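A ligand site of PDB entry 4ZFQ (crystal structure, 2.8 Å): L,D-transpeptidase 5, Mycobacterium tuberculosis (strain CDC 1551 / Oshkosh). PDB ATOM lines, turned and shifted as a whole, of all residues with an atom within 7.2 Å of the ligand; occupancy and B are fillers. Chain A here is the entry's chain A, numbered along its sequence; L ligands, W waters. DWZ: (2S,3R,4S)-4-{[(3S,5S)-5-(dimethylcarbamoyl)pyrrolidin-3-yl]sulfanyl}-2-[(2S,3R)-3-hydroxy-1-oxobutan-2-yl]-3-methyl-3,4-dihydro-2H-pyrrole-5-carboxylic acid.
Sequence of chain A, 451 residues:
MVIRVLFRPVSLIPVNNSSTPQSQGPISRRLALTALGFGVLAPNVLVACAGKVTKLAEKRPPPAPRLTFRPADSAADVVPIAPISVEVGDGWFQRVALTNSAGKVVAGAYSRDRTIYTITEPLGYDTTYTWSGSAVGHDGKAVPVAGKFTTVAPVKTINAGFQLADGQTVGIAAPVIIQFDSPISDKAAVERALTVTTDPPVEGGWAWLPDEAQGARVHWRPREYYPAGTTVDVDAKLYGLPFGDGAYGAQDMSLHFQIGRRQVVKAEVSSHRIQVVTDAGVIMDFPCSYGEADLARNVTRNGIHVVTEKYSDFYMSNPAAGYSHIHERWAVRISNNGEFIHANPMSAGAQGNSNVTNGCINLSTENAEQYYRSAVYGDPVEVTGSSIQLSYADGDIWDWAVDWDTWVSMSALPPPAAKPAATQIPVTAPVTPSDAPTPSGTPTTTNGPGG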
ATOM      1  N   GLY A 291      26.029 -19.007  11.738  1.00  0.00           N
ATOM      2  CA  GLY A 291      25.403 -20.138  11.101  1.00  0.00           C
ATOM      3  C   GLY A 291      26.455 -21.104  10.569  1.00  0.00           C
ATOM      4  O   GLY A 291      27.292 -20.729   9.755  1.00  0.00           O
ATOM      5  N   ALA A 296      22.760 -25.419   3.690  1.00  0.00           N
ATOM      6  CA  ALA A 296      22.830 -24.098   3.062  1.00  0.00           C
ATOM      7  C   ALA A 296      21.665 -23.171   3.456  1.00  0.00           C
ATOM      8  O   ALA A 296      21.638 -22.005   3.061  1.00  0.00           O
ATOM      9  CB  ALA A 296      22.904 -24.259   1.547  1.00  0.00           C
ATOM     10  N   ARG A 297      20.710 -23.705   4.219  1.00  0.00           N
ATOM     11  CA  ARG A 297      19.646 -22.888   4.813  1.00  0.00           C
ATOM     12  C   ARG A 297      20.199 -22.160   6.042  1.00  0.00           C
ATOM     13  O   ARG A 297      19.606 -21.193   6.538  1.00  0.00           O
ATOM     14  CB  ARG A 297      18.444 -23.740   5.253  1.00  0.00           C
ATOM     15  CG  ARG A 297      18.311 -25.126   4.626  1.00  0.00           C
ATOM     16  CD  ARG A 297      17.429 -26.015   5.481  1.00  0.00           C
ATOM     17  NE  ARG A 297      17.190 -27.336   4.879  1.00  0.00           N
ATOM     18  CZ  ARG A 297      16.233 -27.603   3.989  1.00  0.00           C
ATOM     19  NH1 ARG A 297      15.409 -26.652   3.562  1.00  0.00           N
ATOM     20  NH2 ARG A 297      16.103 -28.837   3.526  1.00  0.00           N
ATOM     21  N   ASN A 298      21.356 -22.644   6.501  1.00  0.00           N
ATOM     22  CA  ASN A 298      21.945 -22.316   7.804  1.00  0.00           C
ATOM     23  C   ASN A 298      23.407 -21.858   7.678  1.00  0.00           C
ATOM     24  O   ASN A 298      24.260 -22.260   8.463  1.00  0.00           O
ATOM     25  CB  ASN A 298      21.854 -23.540   8.727  1.00  0.00           C
ATOM     26  CG  ASN A 298      20.451 -23.774   9.286  1.00  0.00           C
ATOM     27  OD1 ASN A 298      19.892 -24.866   9.130  1.00  0.00           O
ATOM     28  ND2 ASN A 298      19.889 -22.762   9.936  1.00  0.00           N
ATOM     29  N   VAL A 299      23.680 -21.030   6.682  1.00  0.00           N
ATOM     30  CA  VAL A 299      24.965 -20.347   6.600  1.00  0.00           C
ATOM     31  C   VAL A 299      24.713 -18.869   6.598  1.00  0.00           C
ATOM     32  O   VAL A 299      23.952 -18.361   5.768  1.00  0.00           O
ATOM     33  CB  VAL A 299      25.768 -20.699   5.326  1.00  0.00           C
ATOM     34  CG1 VAL A 299      27.245 -20.483   5.572  1.00  0.00           C
ATOM     35  CG2 VAL A 299      25.510 -22.115   4.888  1.00  0.00           C
ATOM     36  N   THR A 300      25.318 -18.152   7.532  1.00  0.00           N
ATOM     37  CA  THR A 300      25.257 -16.708   7.483  1.00  0.00           C
ATOM     38  C   THR A 300      25.860 -16.279   6.153  1.00  0.00           C
ATOM     39  O   THR A 300      27.010 -16.606   5.846  1.00  0.00           O
ATOM     40  CB  THR A 300      25.988 -16.053   8.663  1.00  0.00           C
ATOM     41  OG1 THR A 300      25.447 -16.592   9.871  1.00  0.00           O
ATOM     42  CG2 THR A 300      25.797 -14.551   8.666  1.00  0.00           C
ATOM     43  N   ARG A 301      25.075 -15.568   5.347  1.00  0.00           N
ATOM     44  CA  ARG A 301      25.478 -15.256   3.991  1.00  0.00           C
ATOM     45  C   ARG A 301      26.705 -14.335   4.017  1.00  0.00           C
ATOM     46  O   ARG A 301      26.968 -13.676   5.018  1.00  0.00           O
ATOM     47  CB  ARG A 301      24.317 -14.612   3.228  1.00  0.00           C
ATOM     48  CG  ARG A 301      23.050 -15.506   3.137  1.00  0.00           C
ATOM     49  CD  ARG A 301      23.166 -16.571   2.074  1.00  0.00           C
ATOM     50  NE  ARG A 301      21.885 -17.223   1.824  1.00  0.00           N
ATOM     51  CZ  ARG A 301      21.504 -18.389   2.321  1.00  0.00           C
ATOM     52  NH1 ARG A 301      22.308 -19.112   3.107  1.00  0.00           N
ATOM     53  NH2 ARG A 301      20.307 -18.871   2.015  1.00  0.00           N
ATOM     54  N   MET A 316       8.137 -14.274  15.137  1.00  0.00           N
ATOM     55  CA  MET A 316       8.297 -14.569  13.712  1.00  0.00           C
ATOM     56  C   MET A 316       8.261 -16.085  13.460  1.00  0.00           C
ATOM     57  O   MET A 316       9.186 -16.813  13.849  1.00  0.00           O
ATOM     58  CB  MET A 316       9.609 -13.954  13.203  1.00  0.00           C
ATOM     59  CG  MET A 316       9.862 -14.118  11.699  1.00  0.00           C
ATOM     60  SD  MET A 316      11.415 -13.367  11.147  1.00  0.00           S
ATOM     61  CE  MET A 316      11.637 -14.167   9.558  1.00  0.00           C
ATOM     62  N   ASN A 318       9.076 -18.537  11.190  1.00  0.00           N
ATOM     63  CA  ASN A 318      10.055 -18.579  10.079  1.00  0.00           C
ATOM     64  C   ASN A 318       9.680 -19.321   8.789  1.00  0.00           C
ATOM     65  O   ASN A 318       8.657 -20.002   8.724  1.00  0.00           O
ATOM     66  CB  ASN A 318      11.357 -19.186  10.604  1.00  0.00           C
ATOM     67  CG  ASN A 318      11.865 -18.495  11.835  1.00  0.00           C
ATOM     68  OD1 ASN A 318      12.510 -19.115  12.694  1.00  0.00           O
ATOM     69  ND2 ASN A 318      11.584 -17.204  11.956  1.00  0.00           N
ATOM     70  N   PRO A 319      10.537 -19.190   7.750  1.00  0.00           N
ATOM     71  CA  PRO A 319      10.396 -19.925   6.489  1.00  0.00           C
ATOM     72  C   PRO A 319      10.188 -21.422   6.688  1.00  0.00           C
ATOM     73  O   PRO A 319       9.906 -22.130   5.718  1.00  0.00           O
ATOM     74  CB  PRO A 319      11.749 -19.670   5.778  1.00  0.00           C
ATOM     75  CG  PRO A 319      12.661 -19.061   6.832  1.00  0.00           C
ATOM     76  CD  PRO A 319      11.719 -18.310   7.728  1.00  0.00           C
ATOM     77  N   GLU A 328      11.957 -13.713  19.187  1.00  0.00           N
ATOM     78  CA  GLU A 328      13.281 -13.150  19.420  1.00  0.00           C
ATOM     79  C   GLU A 328      13.335 -12.053  20.482  1.00  0.00           C
ATOM     80  O   GLU A 328      12.332 -11.401  20.772  1.00  0.00           O
ATOM     81  CB  GLU A 328      13.845 -12.589  18.123  1.00  0.00           C
ATOM     82  CG  GLU A 328      14.541 -13.640  17.260  1.00  0.00           C
ATOM     83  CD  GLU A 328      14.099 -13.632  15.800  1.00  0.00           C
ATOM     84  OE1 GLU A 328      12.928 -13.254  15.526  1.00  0.00           O
ATOM     85  OE2 GLU A 328      14.918 -14.004  14.937  1.00  0.00           O
ATOM     86  N   ARG A 333      17.614  -6.787  12.357  1.00  0.00           N
ATOM     87  CA  ARG A 333      17.585  -7.453  11.050  1.00  0.00           C
ATOM     88  C   ARG A 333      18.764  -6.985  10.205  1.00  0.00           C
ATOM     89  O   ARG A 333      19.042  -5.785  10.144  1.00  0.00           O
ATOM     90  CB  ARG A 333      16.268  -7.186  10.322  1.00  0.00           C
ATOM     91  CG  ARG A 333      16.198  -7.739   8.905  1.00  0.00           C
ATOM     92  CD  ARG A 333      14.816  -7.474   8.208  1.00  0.00           C
ATOM     93  NE  ARG A 333      13.715  -8.265   8.772  1.00  0.00           N
ATOM     94  CZ  ARG A 333      13.543  -9.562   8.544  1.00  0.00           C
ATOM     95  NH1 ARG A 333      14.395 -10.222   7.753  1.00  0.00           N
ATOM     96  NH2 ARG A 333      12.526 -10.208   9.098  1.00  0.00           N
ATOM     97  N   ASN A 336      16.486  -9.533   4.615  1.00  0.00           N
ATOM     98  CA  ASN A 336      15.129 -10.030   4.454  1.00  0.00           C
ATOM     99  C   ASN A 336      15.081 -11.560   4.349  1.00  0.00           C
ATOM    100  O   ASN A 336      13.995 -12.151   4.278  1.00  0.00           O
ATOM    101  CB  ASN A 336      14.479  -9.410   3.225  1.00  0.00           C
ATOM    102  CG  ASN A 336      14.007  -7.954   3.443  1.00  0.00           C
ATOM    103  OD1 ASN A 336      14.064  -7.412   4.567  1.00  0.00           O
ATOM    104  ND2 ASN A 336      13.531  -7.332   2.367  1.00  0.00           N
ATOM    105  N   ASN A 337      16.243 -12.212   4.310  1.00  0.00           N
ATOM    106  CA  ASN A 337      16.275 -13.677   4.369  1.00  0.00           C
ATOM    107  C   ASN A 337      15.965 -14.168   5.771  1.00  0.00           C
ATOM    108  O   ASN A 337      15.800 -15.359   5.996  1.00  0.00           O
ATOM    109  CB  ASN A 337      17.624 -14.242   3.906  1.00  0.00           C
ATOM    110  CG  ASN A 337      18.800 -13.780   4.778  1.00  0.00           C
ATOM    111  OD1 ASN A 337      18.650 -13.485   5.961  1.00  0.00           O
ATOM    112  ND2 ASN A 337      19.995 -13.718   4.175  1.00  0.00           N
ATOM    113  N   GLY A 338      15.913 -13.237   6.718  1.00  0.00           N
ATOM    114  CA  GLY A 338      15.621 -13.560   8.095  1.00  0.00           C
ATOM    115  C   GLY A 338      16.850 -13.701   8.952  1.00  0.00           C
ATOM    116  O   GLY A 338      16.795 -14.325  10.015  1.00  0.00           O
ATOM    117  N   GLU A 339      17.969 -13.143   8.498  1.00  0.00           N
ATOM    118  CA  GLU A 339      19.179 -13.102   9.314  1.00  0.00           C
ATOM    119  C   GLU A 339      19.129 -11.949  10.301  1.00  0.00           C
ATOM    120  O   GLU A 339      18.838 -10.806   9.938  1.00  0.00           O
ATOM    121  CB  GLU A 339      20.420 -12.975   8.433  1.00  0.00           C
ATOM    122  CG  GLU A 339      20.860 -14.290   7.895  1.00  0.00           C
ATOM    123  CD  GLU A 339      21.885 -14.169   6.795  1.00  0.00           C
ATOM    124  OE1 GLU A 339      22.367 -13.049   6.537  1.00  0.00           O
ATOM    125  OE2 GLU A 339      22.222 -15.212   6.201  1.00  0.00           O
ATOM    126  N   PHE A 340      19.429 -12.267  11.551  1.00  0.00           N
ATOM    127  CA  PHE A 340      19.396 -11.292  12.629  1.00  0.00           C
ATOM    128  C   PHE A 340      20.655 -11.351  13.464  1.00  0.00           C
ATOM    129  O   PHE A 340      21.424 -12.306  13.391  1.00  0.00           O
ATOM    130  CB  PHE A 340      18.190 -11.530  13.527  1.00  0.00           C
ATOM    131  CG  PHE A 340      16.876 -11.151  12.904  1.00  0.00           C
ATOM    132  CD1 PHE A 340      16.201 -10.006  13.313  1.00  0.00           C
ATOM    133  CD2 PHE A 340      16.299 -11.943  11.933  1.00  0.00           C
ATOM    134  CE1 PHE A 340      14.988  -9.666  12.736  1.00  0.00           C
ATOM    135  CE2 PHE A 340      15.105 -11.610  11.357  1.00  0.00           C
ATOM    136  CZ  PHE A 340      14.442 -10.461  11.759  1.00  0.00           C
ATOM    137  N   HIS A 342      20.931 -11.242  17.453  1.00  0.00           N
ATOM    138  CA  HIS A 342      19.981 -11.270  18.563  1.00  0.00           C
ATOM    139  C   HIS A 342      20.457 -12.158  19.674  1.00  0.00           C
ATOM    140  O   HIS A 342      21.624 -12.516  19.707  1.00  0.00           O
ATOM    141  CB  HIS A 342      18.602 -11.719  18.063  1.00  0.00           C
ATOM    142  CG  HIS A 342      18.574 -13.081  17.429  1.00  0.00           C
ATOM    143  ND1 HIS A 342      19.154 -14.191  17.996  1.00  0.00           N
ATOM    144  CD2 HIS A 342      18.008 -13.504  16.278  1.00  0.00           C
ATOM    145  CE1 HIS A 342      18.945 -15.239  17.225  1.00  0.00           C
ATOM    146  NE2 HIS A 342      18.248 -14.849  16.173  1.00  0.00           N
ATOM    147  N   ASN A 344      19.949 -15.767  22.014  1.00  0.00           N
ATOM    148  CA  ASN A 344      19.357 -17.104  22.069  1.00  0.00           C
ATOM    149  C   ASN A 344      20.265 -18.043  22.850  1.00  0.00           C
ATOM    150  O   ASN A 344      21.484 -17.833  22.874  1.00  0.00           O
ATOM    151  CB  ASN A 344      19.097 -17.628  20.649  1.00  0.00           C
ATOM    152  CG  ASN A 344      17.749 -18.308  20.493  1.00  0.00           C
ATOM    153  OD1 ASN A 344      16.854 -18.154  21.318  1.00  0.00           O
ATOM    154  ND2 ASN A 344      17.592 -19.067  19.415  1.00  0.00           N
ATOM    155  N   THR A 357      24.203 -23.742  15.930  1.00  0.00           N
ATOM    156  CA  THR A 357      24.942 -22.662  15.295  1.00  0.00           C
ATOM    157  C   THR A 357      23.998 -21.848  14.349  1.00  0.00           C
ATOM    158  O   THR A 357      23.933 -20.608  14.446  1.00  0.00           O
ATOM    159  CB  THR A 357      26.206 -23.231  14.578  1.00  0.00           C
ATOM    160  OG1 THR A 357      26.176 -24.660  14.636  1.00  0.00           O
ATOM    161  CG2 THR A 357      27.503 -22.776  15.279  1.00  0.00           C
ATOM    162  N   ASN A 358      23.275 -22.534  13.445  1.00  0.00           N
ATOM    163  CA  ASN A 358      22.065 -22.020  12.736  1.00  0.00           C
ATOM    164  C   ASN A 358      22.272 -21.078  11.515  1.00  0.00           C
ATOM    165  O   ASN A 358      23.002 -21.438  10.598  1.00  0.00           O
ATOM    166  CB  ASN A 358      21.123 -21.345  13.749  1.00  0.00           C
ATOM    167  CG  ASN A 358      19.670 -21.342  13.275  1.00  0.00           C
ATOM    168  OD1 ASN A 358      19.395 -21.187  12.088  1.00  0.00           O
ATOM    169  ND2 ASN A 358      18.745 -21.531  14.207  1.00  0.00           N
ATOM    170  N   GLY A 359      21.563 -19.938  11.445  1.00  0.00           N
ATOM    171  CA  GLY A 359      21.725 -18.988  10.334  1.00  0.00           C
ATOM    172  C   GLY A 359      21.965 -17.559  10.794  1.00  0.00           C
ATOM    173  O   GLY A 359      22.650 -16.752  10.148  1.00  0.00           O
ATOM    174  N   CYS A 360      21.367 -17.217  11.931  1.00  0.00           N
ATOM    175  CA  CYS A 360      21.556 -15.916  12.536  1.00  0.00           C
ATOM    176  C   CYS A 360      22.969 -15.809  13.127  1.00  0.00           C
ATOM    177  O   CYS A 360      23.850 -16.598  12.821  1.00  0.00           O
ATOM    178  CB  CYS A 360      20.514 -15.663  13.633  1.00  0.00           C
ATOM    179  SG  CYS A 360      18.772 -15.794  13.091  1.00  0.00           S
ATOM    180  N   ILE A 361      23.123 -14.815  13.983  1.00  0.00           N
ATOM    181  CA  ILE A 361      24.345 -14.484  14.687  1.00  0.00           C
ATOM    182  C   ILE A 361      24.014 -14.335  16.157  1.00  0.00           C
ATOM    183  O   ILE A 361      23.580 -13.260  16.563  1.00  0.00           O
ATOM    184  CB  ILE A 361      24.911 -13.157  14.168  1.00  0.00           C
ATOM    185  CG1 ILE A 361      25.338 -13.303  12.712  1.00  0.00           C
ATOM    186  CG2 ILE A 361      26.070 -12.652  15.048  1.00  0.00           C
ATOM    187  CD1 ILE A 361      25.869 -11.994  12.111  1.00  0.00           C
ATOM    188  N   ASN A 362      24.196 -15.374  16.951  1.00  0.00           N
ATOM    189  CA  ASN A 362      23.687 -15.412  18.329  1.00  0.00           C
ATOM    190  C   ASN A 362      24.573 -14.726  19.378  1.00  0.00           C
ATOM    191  O   ASN A 362      25.782 -14.904  19.409  1.00  0.00           O
ATOM    192  CB  ASN A 362      23.431 -16.863  18.755  1.00  0.00           C
ATOM    193  CG  ASN A 362      22.280 -17.514  17.981  1.00  0.00           C
ATOM    194  OD1 ASN A 362      21.181 -17.703  18.520  1.00  0.00           O
ATOM    195  ND2 ASN A 362      22.517 -17.871  16.722  1.00  0.00           N
ATOM    196  N   ASP A 394      18.306 -13.320  -1.288  1.00  0.00           N
ATOM    197  CA  ASP A 394      18.205 -13.099   0.143  1.00  0.00           C
ATOM    198  C   ASP A 394      17.283 -11.943   0.458  1.00  0.00           C
ATOM    199  O   ASP A 394      16.833 -11.781   1.602  1.00  0.00           O
ATOM    200  CB  ASP A 394      19.587 -12.868   0.732  1.00  0.00           C
ATOM    201  CG  ASP A 394      20.427 -14.104   0.677  1.00  0.00           C
ATOM    202  OD1 ASP A 394      21.221 -14.288  -0.284  1.00  0.00           O
ATOM    203  OD2 ASP A 394      20.263 -14.934   1.595  1.00  0.00           O
HETATM  204  SAK DWZ L   1      15.899 -20.578   8.147  1.00  0.00           S
HETATM  205  CAI DWZ L   1      16.042 -18.697   8.426  1.00  0.00           C
HETATM  206  CAH DWZ L   1      15.478 -18.201   9.771  1.00  0.00           C
HETATM  207  CAS DWZ L   1      14.818 -16.816   9.604  1.00  0.00           C
HETATM  208  CAL DWZ L   1      17.527 -18.358   8.501  1.00  0.00           C
HETATM  209  CAM DWZ L   1      18.476 -18.376   7.311  1.00  0.00           C
HETATM  210  OAT DWZ L   1      19.685 -18.626   7.494  1.00  0.00           O
HETATM  211  OAU DWZ L   1      18.041 -18.160   6.139  1.00  0.00           O
HETATM  212  NAJ DWZ L   1      17.944 -18.052   9.693  1.00  0.00           N
HETATM  213  CAD DWZ L   1      16.774 -18.159  10.579  1.00  0.00           C
HETATM  214  CAB DWZ L   1      16.791 -17.325  11.801  1.00  0.00           C
HETATM  215  CAE DWZ L   1      15.801 -17.832  12.869  1.00  0.00           C
HETATM  216  CAF DWZ L   1      16.369 -18.917  13.685  1.00  0.00           C
HETATM  217  OAG DWZ L   1      15.435 -16.747  13.740  1.00  0.00           O
HETATM  218  CAA DWZ L   1      18.209 -17.295  12.402  1.00  0.00           C
HETATM  219  OAC DWZ L   1      18.915 -18.271  12.402  1.00  0.00           O
HETATM  220  O   HOH W   1      21.469 -17.515   6.281  1.00  0.00           O
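The backbone NH (N) of Cys 360 sits at hydrogen-bond distance from an oxygen (OAC) of the ligand, at 2.7 Å. SG of Cys 360 is bonded to CAA of the ligand. The backbone carbonyl oxygen (O) of Arg 297 sits close to an oxygen (OAT) of the ligand (2.7 Å). OD1 of Asn 358 lies close to OAC of the ligand. The side-chain carboxylate (OE2) of Glu 328 is in hydrogen-bond range of an oxygen (OAG) of the ligand (3.0 Å). An oxygen (OAC) of the ligand lies within hydrogen-bond range of the backbone NH (N) of Gly 359, 3.3 Å away.
SG of Cys 360 is in hydrogen-bond range of NE2 of His 342, 3.3 Å away. O of Cys 360 is in hydrogen-bond range of OG1 of Thr 300, 3.4 Å away. The backbone carbonyl oxygen (O) of Cys 360 is in hydrogen-bond range of the backbone NH (N) of Gly 291 (3.4 Å). The side-chain amide nitrogen (ND2) of Asn 298 is in hydrogen-bond range of the side-chain amide oxygen (OD1) of Asn 358 (2.7 Å). The backbone carbonyl oxygen (O) of Gly 359 is in hydrogen-bond range of the side-chain hydroxyl (OG1) of Thr 300 (2.8 Å). The side-chain amide nitrogen of Asn 318 lies within hydrogen-bond range of the backbone carbonyl oxygen of Met 316, 3.1 Å away. The backbone NH (N) of Glu 339 sits at hydrogen-bond distance from the side-chain amide oxygen (OD1) of Asn 337, at 2.6 Å. N of Asn 337 lies within hydrogen-bond range of O of Asp 394, 2.8 Å away.
Residues that only touch the ligand: Asn 318, Pro 319, Asn 337 and Gly 338. Hydrophobic or aromatic side chains within 4 Å of the ligand: Pro 319. Within 4 Å of the ligand: Arg 297, Asn 318, Pro 319, Glu 328, Asn 337, Gly 338, Asn 358, Gly 359 and Cys 360.
Water W1 lies within hydrogen-bond range of OE2 of Glu 339 (2.4 Å), OAT of the ligand (2.4 Å) and O of Val 299 (2.7 Å).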
